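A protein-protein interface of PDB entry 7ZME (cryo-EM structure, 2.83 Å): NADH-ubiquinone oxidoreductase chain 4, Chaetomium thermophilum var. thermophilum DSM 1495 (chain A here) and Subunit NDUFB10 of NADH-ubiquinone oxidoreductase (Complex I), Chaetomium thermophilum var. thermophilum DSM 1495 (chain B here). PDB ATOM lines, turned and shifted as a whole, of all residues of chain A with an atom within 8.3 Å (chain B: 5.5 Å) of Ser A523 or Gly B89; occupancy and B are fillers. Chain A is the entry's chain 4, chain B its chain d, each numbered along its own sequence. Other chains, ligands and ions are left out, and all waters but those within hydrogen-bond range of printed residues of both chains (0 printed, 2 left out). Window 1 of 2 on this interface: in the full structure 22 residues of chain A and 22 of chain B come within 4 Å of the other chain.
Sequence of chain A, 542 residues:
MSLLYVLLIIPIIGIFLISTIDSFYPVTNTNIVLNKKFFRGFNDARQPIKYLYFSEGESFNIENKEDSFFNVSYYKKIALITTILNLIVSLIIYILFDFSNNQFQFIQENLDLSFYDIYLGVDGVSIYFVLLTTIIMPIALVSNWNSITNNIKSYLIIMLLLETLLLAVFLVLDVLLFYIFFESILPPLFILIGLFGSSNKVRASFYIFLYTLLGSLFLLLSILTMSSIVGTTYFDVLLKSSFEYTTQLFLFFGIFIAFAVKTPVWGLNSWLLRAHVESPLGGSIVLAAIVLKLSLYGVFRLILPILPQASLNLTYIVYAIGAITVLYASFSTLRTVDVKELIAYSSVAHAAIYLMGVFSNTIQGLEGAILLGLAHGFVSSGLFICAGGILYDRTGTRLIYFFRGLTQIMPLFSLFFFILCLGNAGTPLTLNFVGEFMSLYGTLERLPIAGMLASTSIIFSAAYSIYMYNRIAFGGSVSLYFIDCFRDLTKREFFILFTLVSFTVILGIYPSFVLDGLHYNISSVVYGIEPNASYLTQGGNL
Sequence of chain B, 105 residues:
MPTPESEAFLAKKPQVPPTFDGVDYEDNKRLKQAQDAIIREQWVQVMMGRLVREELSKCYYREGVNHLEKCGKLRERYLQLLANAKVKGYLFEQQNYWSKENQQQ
Of the 20 printed residues of chain A, 8 touch a printed residue of chain B.
Hydrophobic or aromatic side chains of chain B that line the printed part of chain A: Ile B39, Trp B43, Val B87, Tyr B90, Leu B91 and Phe B92.
Among the printed residues, 16 pairs touch across the chains.
Among the printed residues, no Asp or Glu carboxylate lies within 4 Å of a Lys or Arg side-chain nitrogen of the other chain.
Among the printed residues, merely in contact across the chains: Ser A523 with Gly B89 (3.1 Å), Tyr A527 with Phe B92 (3.3 Å), Ser A524 with Tyr B90 (3.4 Å), Ser A523 with Ile B39 (3.6 Å), Ile A363 with Trp B43 (3.6 Å), Ile A529 with Phe B92 (3.6 Å), Ile A363 with Val B87 (3.7 Å), Ser A523 with Val B87 (3.7 Å), Val A526 with Leu B91 (3.7 Å), His A519 with Trp B43 (3.8 Å), Ile A529 with Lys B88 (3.8 Å), Gly A528 with Phe B92 (3.9 Å) and Tyr A527 with Lys B88 (3.9 Å).
The side-chain amide nitrogen of Gln B42 lies within hydrogen-bond range of the backbone carbonyl oxygen of Gly B89 (3.1 Å).
The side-chain amide nitrogen (ND2) of Asn A361 lies within hydrogen-bond range of the backbone carbonyl oxygen (O) of Tyr A527 (2.7 Å).
The side-chain carboxylate (OE2) of Glu A367 sits at hydrogen-bond distance from a ring nitrogen (ND1) of His A519 (2.7 Å).
The backbone carbonyl oxygen of His A519 is in hydrogen-bond range of the side-chain hydroxyl of Ser A523.
OG of Ser A523 sits close to O of Tyr A520 (3.4 Å).
Of the printed residues of chain B, Ser A523 touches Ile B39, Trp B43, Val B87 and Gly B89.
Gly B89 touches one residue of chain A.
Printed residues of chain A within 4 Å of Lys B88: Val A526 (3.4 Å), Tyr A527 (3.9 Å), Gly A528 (3.2 Å) and Ile A529 (3.8 Å).
Of the printed residues of chain A, Phe B92 touches Tyr A527 (3.3 Å), Gly A528 (3.9 Å) and Ile A529 (3.6 Å).
Printed residues of chain A within 4 Å of Ile B39: Ser A523 (3.6 Å).
The nearest residue of chain A that does not touch Gly B89 is Val A526 (4.2 Å).
The indole nitrogen of Trp B43 is in hydrogen-bond range of the side-chain hydroxyl of Ser A523.
The backbone carbonyl oxygen of Val A526 lies close to the backbone carbonyl oxygen of Lys B88.
The backbone carbonyl oxygen (O) of Gly A528 lies close to the backbone carbonyl oxygen (O) of Lys B88.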
ATOM      1  N   PHE A 300     -35.336 -25.970  14.778  1.00  0.00           N
ATOM      2  CA  PHE A 300     -35.212 -25.447  13.426  1.00  0.00           C
ATOM      3  C   PHE A 300     -35.041 -23.936  13.383  1.00  0.00           C
ATOM      4  O   PHE A 300     -34.717 -23.398  12.320  1.00  0.00           O
ATOM      5  CB  PHE A 300     -36.436 -25.847  12.599  1.00  0.00           C
ATOM      6  CG  PHE A 300     -36.402 -27.267  12.120  1.00  0.00           C
ATOM      7  CD1 PHE A 300     -35.659 -27.621  11.011  1.00  0.00           C
ATOM      8  CD2 PHE A 300     -37.108 -28.252  12.783  1.00  0.00           C
ATOM      9  CE1 PHE A 300     -35.620 -28.928  10.577  1.00  0.00           C
ATOM     10  CE2 PHE A 300     -37.075 -29.559  12.348  1.00  0.00           C
ATOM     11  CZ  PHE A 300     -36.331 -29.897  11.245  1.00  0.00           C
ATOM     12  N   ASN A 361     -28.205 -33.801  11.007  1.00  0.00           N
ATOM     13  CA  ASN A 361     -27.475 -32.989   9.996  1.00  0.00           C
ATOM     14  C   ASN A 361     -27.686 -33.678   8.651  1.00  0.00           C
ATOM     15  O   ASN A 361     -26.821 -33.567   7.773  1.00  0.00           O
ATOM     16  CB  ASN A 361     -26.032 -32.680  10.402  1.00  0.00           C
ATOM     17  CG  ASN A 361     -25.471 -31.432   9.764  1.00  0.00           C
ATOM     18  OD1 ASN A 361     -26.215 -30.572   9.313  1.00  0.00           O
ATOM     19  ND2 ASN A 361     -24.155 -31.325   9.743  1.00  0.00           N
ATOM     20  N   ILE A 363     -30.669 -34.365   5.570  1.00  0.00           N
ATOM     21  CA  ILE A 363     -31.935 -33.892   5.031  1.00  0.00           C
ATOM     22  C   ILE A 363     -33.029 -34.934   5.213  1.00  0.00           C
ATOM     23  O   ILE A 363     -34.208 -34.590   5.352  1.00  0.00           O
ATOM     24  CB  ILE A 363     -31.752 -33.494   3.553  1.00  0.00           C
ATOM     25  CG1 ILE A 363     -32.976 -32.732   3.040  1.00  0.00           C
ATOM     26  CG2 ILE A 363     -31.433 -34.704   2.713  1.00  0.00           C
ATOM     27  CD1 ILE A 363     -32.693 -31.870   1.855  1.00  0.00           C
ATOM     28  N   LEU A 366     -33.868 -34.883   9.188  1.00  0.00           N
ATOM     29  CA  LEU A 366     -34.583 -33.670   9.566  1.00  0.00           C
ATOM     30  C   LEU A 366     -36.026 -33.709   9.087  1.00  0.00           C
ATOM     31  O   LEU A 366     -36.943 -33.321   9.818  1.00  0.00           O
ATOM     32  CB  LEU A 366     -33.868 -32.447   9.001  1.00  0.00           C
ATOM     33  CG  LEU A 366     -32.488 -32.137   9.571  1.00  0.00           C
ATOM     34  CD1 LEU A 366     -31.691 -31.287   8.608  1.00  0.00           C
ATOM     35  CD2 LEU A 366     -32.627 -31.451  10.904  1.00  0.00           C
ATOM     36  N   GLU A 367     -36.245 -34.167   7.855  1.00  0.00           N
ATOM     37  CA  GLU A 367     -37.599 -34.246   7.323  1.00  0.00           C
ATOM     38  C   GLU A 367     -38.407 -35.321   8.031  1.00  0.00           C
ATOM     39  O   GLU A 367     -39.552 -35.083   8.428  1.00  0.00           O
ATOM     40  CB  GLU A 367     -37.548 -34.505   5.822  1.00  0.00           C
ATOM     41  CG  GLU A 367     -37.123 -33.289   5.039  1.00  0.00           C
ATOM     42  CD  GLU A 367     -37.438 -33.390   3.578  1.00  0.00           C
ATOM     43  OE1 GLU A 367     -38.476 -32.845   3.154  1.00  0.00           O
ATOM     44  OE2 GLU A 367     -36.640 -34.008   2.846  1.00  0.00           O
ATOM     45  N   LEU A 518     -41.545 -29.324   2.236  1.00  0.00           N
ATOM     46  CA  LEU A 518     -40.564 -29.377   3.300  1.00  0.00           C
ATOM     47  C   LEU A 518     -39.135 -29.476   2.787  1.00  0.00           C
ATOM     48  O   LEU A 518     -38.202 -29.183   3.542  1.00  0.00           O
ATOM     49  CB  LEU A 518     -40.874 -30.574   4.208  1.00  0.00           C
ATOM     50  CG  LEU A 518     -40.583 -30.512   5.703  1.00  0.00           C
ATOM     51  CD1 LEU A 518     -41.471 -29.505   6.401  1.00  0.00           C
ATOM     52  CD2 LEU A 518     -40.754 -31.890   6.313  1.00  0.00           C
ATOM     53  N   HIS A 519     -38.944 -29.849   1.523  1.00  0.00           N
ATOM     54  CA  HIS A 519     -37.630 -30.143   0.967  1.00  0.00           C
ATOM     55  C   HIS A 519     -36.733 -28.922   0.846  1.00  0.00           C
ATOM     56  O   HIS A 519     -35.569 -28.975   1.260  1.00  0.00           O
ATOM     57  CB  HIS A 519     -37.790 -30.776  -0.417  1.00  0.00           C
ATOM     58  CG  HIS A 519     -38.168 -32.222  -0.381  1.00  0.00           C
ATOM     59  ND1 HIS A 519     -37.699 -33.091   0.578  1.00  0.00           N
ATOM     60  CD2 HIS A 519     -38.990 -32.947  -1.174  1.00  0.00           C
ATOM     61  CE1 HIS A 519     -38.204 -34.293   0.363  1.00  0.00           C
ATOM     62  NE2 HIS A 519     -38.984 -34.233  -0.698  1.00  0.00           N
ATOM     63  N   TYR A 520     -37.247 -27.829   0.283  1.00  0.00           N
ATOM     64  CA  TYR A 520     -36.422 -26.670  -0.037  1.00  0.00           C
ATOM     65  C   TYR A 520     -35.989 -25.912   1.212  1.00  0.00           C
ATOM     66  O   TYR A 520     -34.850 -25.441   1.288  1.00  0.00           O
ATOM     67  CB  TYR A 520     -37.187 -25.751  -0.991  1.00  0.00           C
ATOM     68  CG  TYR A 520     -36.490 -24.462  -1.343  1.00  0.00           C
ATOM     69  CD1 TYR A 520     -35.596 -24.402  -2.403  1.00  0.00           C
ATOM     70  CD2 TYR A 520     -36.744 -23.300  -0.634  1.00  0.00           C
ATOM     71  CE1 TYR A 520     -34.961 -23.225  -2.730  1.00  0.00           C
ATOM     72  CE2 TYR A 520     -36.112 -22.122  -0.953  1.00  0.00           C
ATOM     73  CZ  TYR A 520     -35.228 -22.087  -2.002  1.00  0.00           C
ATOM     74  OH  TYR A 520     -34.605 -20.907  -2.318  1.00  0.00           O
ATOM     75  N   ASN A 521     -36.874 -25.782   2.199  1.00  0.00           N
ATOM     76  CA  ASN A 521     -36.554 -24.959   3.360  1.00  0.00           C
ATOM     77  C   ASN A 521     -35.641 -25.677   4.352  1.00  0.00           C
ATOM     78  O   ASN A 521     -34.797 -25.035   4.984  1.00  0.00           O
ATOM     79  CB  ASN A 521     -37.840 -24.493   4.039  1.00  0.00           C
ATOM     80  CG  ASN A 521     -38.423 -23.259   3.385  1.00  0.00           C
ATOM     81  OD1 ASN A 521     -39.574 -23.252   2.962  1.00  0.00           O
ATOM     82  ND2 ASN A 521     -37.622 -22.207   3.292  1.00  0.00           N
ATOM     83  N   ILE A 522     -35.791 -26.994   4.517  1.00  0.00           N
ATOM     84  CA  ILE A 522     -34.854 -27.720   5.368  1.00  0.00           C
ATOM     85  C   ILE A 522     -33.474 -27.803   4.735  1.00  0.00           C
ATOM     86  O   ILE A 522     -32.480 -28.008   5.439  1.00  0.00           O
ATOM     87  CB  ILE A 522     -35.395 -29.118   5.743  1.00  0.00           C
ATOM     88  CG1 ILE A 522     -36.667 -28.993   6.571  1.00  0.00           C
ATOM     89  CG2 ILE A 522     -34.393 -29.935   6.526  1.00  0.00           C
ATOM     90  CD1 ILE A 522     -37.363 -30.284   6.757  1.00  0.00           C
ATOM     91  N   SER A 523     -33.372 -27.595   3.426  1.00  0.00           N
ATOM     92  CA  SER A 523     -32.056 -27.508   2.810  1.00  0.00           C
ATOM     93  C   SER A 523     -31.226 -26.381   3.406  1.00  0.00           C
ATOM     94  O   SER A 523     -29.998 -26.409   3.304  1.00  0.00           O
ATOM     95  CB  SER A 523     -32.203 -27.319   1.304  1.00  0.00           C
ATOM     96  OG  SER A 523     -33.048 -28.315   0.760  1.00  0.00           O
ATOM     97  N   SER A 524     -31.867 -25.400   4.033  1.00  0.00           N
ATOM     98  CA  SER A 524     -31.190 -24.255   4.620  1.00  0.00           C
ATOM     99  C   SER A 524     -30.724 -24.490   6.051  1.00  0.00           C
ATOM    100  O   SER A 524     -30.111 -23.593   6.636  1.00  0.00           O
ATOM    101  CB  SER A 524     -32.108 -23.034   4.584  1.00  0.00           C
ATOM    102  OG  SER A 524     -33.347 -23.312   5.206  1.00  0.00           O
ATOM    103  N   VAL A 525     -30.996 -25.657   6.635  1.00  0.00           N
ATOM    104  CA  VAL A 525     -30.623 -25.922   8.018  1.00  0.00           C
ATOM    105  C   VAL A 525     -29.585 -27.029   8.132  1.00  0.00           C
ATOM    106  O   VAL A 525     -29.308 -27.498   9.234  1.00  0.00           O
ATOM    107  CB  VAL A 525     -31.857 -26.242   8.888  1.00  0.00           C
ATOM    108  CG1 VAL A 525     -32.895 -25.138   8.773  1.00  0.00           C
ATOM    109  CG2 VAL A 525     -32.448 -27.583   8.523  1.00  0.00           C
ATOM    110  N   VAL A 526     -28.997 -27.454   7.015  1.00  0.00           N
ATOM    111  CA  VAL A 526     -27.928 -28.446   7.026  1.00  0.00           C
ATOM    112  C   VAL A 526     -26.596 -27.718   7.115  1.00  0.00           C
ATOM    113  O   VAL A 526     -26.457 -26.584   6.652  1.00  0.00           O
ATOM    114  CB  VAL A 526     -28.000 -29.353   5.780  1.00  0.00           C
ATOM    115  CG1 VAL A 526     -27.076 -30.551   5.928  1.00  0.00           C
ATOM    116  CG2 VAL A 526     -29.420 -29.809   5.536  1.00  0.00           C
ATOM    117  N   TYR A 527     -25.605 -28.370   7.717  1.00  0.00           N
ATOM    118  CA  TYR A 527     -24.288 -27.781   7.942  1.00  0.00           C
ATOM    119  C   TYR A 527     -23.230 -28.709   7.362  1.00  0.00           C
ATOM    120  O   TYR A 527     -22.969 -29.783   7.913  1.00  0.00           O
ATOM    121  CB  TYR A 527     -24.051 -27.539   9.429  1.00  0.00           C
ATOM    122  CG  TYR A 527     -22.834 -26.705   9.737  1.00  0.00           C
ATOM    123  CD1 TYR A 527     -22.714 -25.412   9.250  1.00  0.00           C
ATOM    124  CD2 TYR A 527     -21.804 -27.210  10.519  1.00  0.00           C
ATOM    125  CE1 TYR A 527     -21.603 -24.647   9.532  1.00  0.00           C
ATOM    126  CE2 TYR A 527     -20.693 -26.455  10.807  1.00  0.00           C
ATOM    127  CZ  TYR A 527     -20.596 -25.174  10.313  1.00  0.00           C
ATOM    128  OH  TYR A 527     -19.485 -24.417  10.597  1.00  0.00           O
ATOM    129  N   GLY A 528     -22.621 -28.300   6.263  1.00  0.00           N
ATOM    130  CA  GLY A 528     -21.586 -29.097   5.639  1.00  0.00           C
ATOM    131  C   GLY A 528     -21.397 -28.710   4.193  1.00  0.00           C
ATOM    132  O   GLY A 528     -22.191 -27.975   3.609  1.00  0.00           O
ATOM    133  N   ILE A 529     -20.307 -29.219   3.622  1.00  0.00           N
ATOM    134  CA  ILE A 529     -19.953 -29.001   2.225  1.00  0.00           C
ATOM    135  C   ILE A 529     -19.318 -30.272   1.675  1.00  0.00           C
ATOM    136  O   ILE A 529     -18.909 -31.165   2.417  1.00  0.00           O
ATOM    137  CB  ILE A 529     -18.993 -27.804   2.024  1.00  0.00           C
ATOM    138  CG1 ILE A 529     -17.671 -28.044   2.755  1.00  0.00           C
ATOM    139  CG2 ILE A 529     -19.643 -26.484   2.411  1.00  0.00           C
ATOM    140  CD1 ILE A 529     -16.604 -27.030   2.415  1.00  0.00           C
ATOM    141  N   GLU A 530     -19.246 -30.341   0.355  1.00  0.00           N
ATOM    142  CA  GLU A 530     -18.599 -31.398  -0.400  1.00  0.00           C
ATOM    143  C   GLU A 530     -17.235 -30.931  -0.893  1.00  0.00           C
ATOM    144  O   GLU A 530     -17.030 -29.736  -1.127  1.00  0.00           O
ATOM    145  CB  GLU A 530     -19.449 -31.824  -1.603  1.00  0.00           C
ATOM    146  CG  GLU A 530     -20.796 -32.432  -1.238  1.00  0.00           C
ATOM    147  CD  GLU A 530     -20.684 -33.895  -0.866  1.00  0.00           C
ATOM    148  OE1 GLU A 530     -19.692 -34.538  -1.269  1.00  0.00           O
ATOM    149  OE2 GLU A 530     -21.587 -34.406  -0.173  1.00  0.00           O
ATOM    150  N   ALA A 533     -18.069 -29.756  -4.586  1.00  0.00           N
ATOM    151  CA  ALA A 533     -19.334 -29.094  -4.875  1.00  0.00           C
ATOM    152  C   ALA A 533     -19.486 -27.831  -4.041  1.00  0.00           C
ATOM    153  O   ALA A 533     -20.605 -27.407  -3.738  1.00  0.00           O
ATOM    154  CB  ALA A 533     -20.515 -30.037  -4.642  1.00  0.00           C
ATOM    155  N   SER A 534     -18.366 -27.222  -3.663  1.00  0.00           N
ATOM    156  CA  SER A 534     -18.363 -26.025  -2.839  1.00  0.00           C
ATOM    157  C   SER A 534     -17.385 -25.021  -3.425  1.00  0.00           C
ATOM    158  O   SER A 534     -16.421 -25.393  -4.098  1.00  0.00           O
ATOM    159  CB  SER A 534     -17.979 -26.340  -1.391  1.00  0.00           C
ATOM    160  OG  SER A 534     -16.749 -27.043  -1.340  1.00  0.00           O
ATOM    161  N   ILE B  38     -27.070 -21.324  -4.344  1.00  0.00           N
ATOM    162  CA  ILE B  38     -26.323 -22.451  -3.791  1.00  0.00           C
ATOM    163  C   ILE B  38     -27.217 -23.679  -3.681  1.00  0.00           C
ATOM    164  O   ILE B  38     -26.812 -24.795  -4.025  1.00  0.00           O
ATOM    165  CB  ILE B  38     -25.718 -22.061  -2.428  1.00  0.00           C
ATOM    166  CG1 ILE B  38     -24.519 -21.137  -2.622  1.00  0.00           C
ATOM    167  CG2 ILE B  38     -25.299 -23.290  -1.644  1.00  0.00           C
ATOM    168  CD1 ILE B  38     -23.384 -21.782  -3.361  1.00  0.00           C
ATOM    169  N   ILE B  39     -28.449 -23.488  -3.209  1.00  0.00           N
ATOM    170  CA  ILE B  39     -29.350 -24.610  -2.974  1.00  0.00           C
ATOM    171  C   ILE B  39     -29.815 -25.223  -4.289  1.00  0.00           C
ATOM    172  O   ILE B  39     -29.921 -26.449  -4.410  1.00  0.00           O
ATOM    173  CB  ILE B  39     -30.533 -24.154  -2.101  1.00  0.00           C
ATOM    174  CG1 ILE B  39     -30.029 -23.707  -0.729  1.00  0.00           C
ATOM    175  CG2 ILE B  39     -31.557 -25.259  -1.952  1.00  0.00           C
ATOM    176  CD1 ILE B  39     -29.473 -24.822   0.110  1.00  0.00           C
ATOM    177  N   GLN B  42     -27.102 -27.515  -5.847  1.00  0.00           N
ATOM    178  CA  GLN B  42     -26.999 -28.783  -5.137  1.00  0.00           C
ATOM    179  C   GLN B  42     -28.157 -29.704  -5.490  1.00  0.00           C
ATOM    180  O   GLN B  42     -27.967 -30.912  -5.676  1.00  0.00           O
ATOM    181  CB  GLN B  42     -26.968 -28.532  -3.633  1.00  0.00           C
ATOM    182  CG  GLN B  42     -25.614 -28.203  -3.075  1.00  0.00           C
ATOM    183  CD  GLN B  42     -25.705 -27.683  -1.667  1.00  0.00           C
ATOM    184  OE1 GLN B  42     -26.786 -27.359  -1.179  1.00  0.00           O
ATOM    185  NE2 GLN B  42     -24.567 -27.604  -0.997  1.00  0.00           N
ATOM    186  N   TRP B  43     -29.369 -29.151  -5.576  1.00  0.00           N
ATOM    187  CA  TRP B  43     -30.535 -29.964  -5.893  1.00  0.00           C
ATOM    188  C   TRP B  43     -30.494 -30.488  -7.321  1.00  0.00           C
ATOM    189  O   TRP B  43     -30.996 -31.584  -7.585  1.00  0.00           O
ATOM    190  CB  TRP B  43     -31.814 -29.161  -5.644  1.00  0.00           C
ATOM    191  CG  TRP B  43     -32.305 -29.283  -4.239  1.00  0.00           C
ATOM    192  CD1 TRP B  43     -32.209 -28.350  -3.255  1.00  0.00           C
ATOM    193  CD2 TRP B  43     -32.961 -30.413  -3.654  1.00  0.00           C
ATOM    194  NE1 TRP B  43     -32.762 -28.822  -2.095  1.00  0.00           N
ATOM    195  CE2 TRP B  43     -33.234 -30.088  -2.314  1.00  0.00           C
ATOM    196  CE3 TRP B  43     -33.345 -31.666  -4.136  1.00  0.00           C
ATOM    197  CZ2 TRP B  43     -33.872 -30.971  -1.449  1.00  0.00           C
ATOM    198  CZ3 TRP B  43     -33.981 -32.538  -3.275  1.00  0.00           C
ATOM    199  CH2 TRP B  43     -34.237 -32.188  -1.947  1.00  0.00           C
ATOM    200  N   VAL B  87     -27.288 -32.613  -0.993  1.00  0.00           N
ATOM    201  CA  VAL B  87     -27.803 -31.337  -0.511  1.00  0.00           C
ATOM    202  C   VAL B  87     -27.195 -31.080   0.863  1.00  0.00           C
ATOM    203  O   VAL B  87     -27.541 -31.746   1.841  1.00  0.00           O
ATOM    204  CB  VAL B  87     -29.335 -31.329  -0.461  1.00  0.00           C
ATOM    205  CG1 VAL B  87     -29.843 -30.148   0.352  1.00  0.00           C
ATOM    206  CG2 VAL B  87     -29.902 -31.289  -1.869  1.00  0.00           C
ATOM    207  N   LYS B  88     -26.265 -30.133   0.932  1.00  0.00           N
ATOM    208  CA  LYS B  88     -25.559 -29.823   2.165  1.00  0.00           C
ATOM    209  C   LYS B  88     -25.878 -28.444   2.716  1.00  0.00           C
ATOM    210  O   LYS B  88     -25.433 -28.124   3.821  1.00  0.00           O
ATOM    211  CB  LYS B  88     -24.044 -29.939   1.956  1.00  0.00           C
ATOM    212  CG  LYS B  88     -23.563 -31.322   1.593  1.00  0.00           C
ATOM    213  CD  LYS B  88     -23.823 -32.287   2.723  1.00  0.00           C
ATOM    214  CE  LYS B  88     -22.909 -32.013   3.902  1.00  0.00           C
ATOM    215  NZ  LYS B  88     -23.099 -33.001   4.996  1.00  0.00           N
ATOM    216  N   GLY B  89     -26.622 -27.625   1.984  1.00  0.00           N
ATOM    217  CA  GLY B  89     -27.009 -26.310   2.450  1.00  0.00           C
ATOM    218  C   GLY B  89     -26.088 -25.218   1.945  1.00  0.00           C
ATOM    219  O   GLY B  89     -25.153 -25.442   1.172  1.00  0.00           O
ATOM    220  N   TYR B  90     -26.384 -24.005   2.401  1.00  0.00           N
ATOM    221  CA  TYR B  90     -25.571 -22.830   2.135  1.00  0.00           C
ATOM    222  C   TYR B  90     -24.825 -22.348   3.367  1.00  0.00           C
ATOM    223  O   TYR B  90     -24.022 -21.418   3.267  1.00  0.00           O
ATOM    224  CB  TYR B  90     -26.445 -21.691   1.590  1.00  0.00           C
ATOM    225  CG  TYR B  90     -27.545 -21.217   2.529  1.00  0.00           C
ATOM    226  CD1 TYR B  90     -27.249 -20.542   3.707  1.00  0.00           C
ATOM    227  CD2 TYR B  90     -28.874 -21.441   2.233  1.00  0.00           C
ATOM    228  CE1 TYR B  90     -28.238 -20.120   4.557  1.00  0.00           C
ATOM    229  CE2 TYR B  90     -29.871 -21.010   3.075  1.00  0.00           C
ATOM    230  CZ  TYR B  90     -29.547 -20.354   4.237  1.00  0.00           C
ATOM    231  OH  TYR B  90     -30.539 -19.925   5.083  1.00  0.00           O
ATOM    232  N   LEU B  91     -25.081 -22.949   4.525  1.00  0.00           N
ATOM    233  CA  LEU B  91     -24.697 -22.346   5.792  1.00  0.00           C
ATOM    234  C   LEU B  91     -23.202 -22.438   6.059  1.00  0.00           C
ATOM    235  O   LEU B  91     -22.645 -21.548   6.706  1.00  0.00           O
ATOM    236  CB  LEU B  91     -25.482 -23.004   6.928  1.00  0.00           C
ATOM    237  CG  LEU B  91     -25.525 -22.294   8.277  1.00  0.00           C
ATOM    238  CD1 LEU B  91     -26.105 -20.902   8.122  1.00  0.00           C
ATOM    239  CD2 LEU B  91     -26.353 -23.104   9.250  1.00  0.00           C
ATOM    240  N   PHE B  92     -22.535 -23.490   5.587  1.00  0.00           N
ATOM    241  CA  PHE B  92     -21.102 -23.598   5.840  1.00  0.00           C
ATOM    242  C   PHE B  92     -20.316 -22.621   4.977  1.00  0.00           C
ATOM    243  O   PHE B  92     -19.353 -22.008   5.447  1.00  0.00           O
ATOM    244  CB  PHE B  92     -20.624 -25.032   5.605  1.00  0.00           C
ATOM    245  CG  PHE B  92     -19.245 -25.298   6.134  1.00  0.00           C
ATOM    246  CD1 PHE B  92     -18.126 -25.026   5.366  1.00  0.00           C
ATOM    247  CD2 PHE B  92     -19.065 -25.803   7.407  1.00  0.00           C
ATOM    248  CE1 PHE B  92     -16.861 -25.261   5.855  1.00  0.00           C
ATOM    249  CE2 PHE B  92     -17.800 -26.037   7.902  1.00  0.00           C
ATOM    250  CZ  PHE B  92     -16.698 -25.768   7.125  1.00  0.00           C
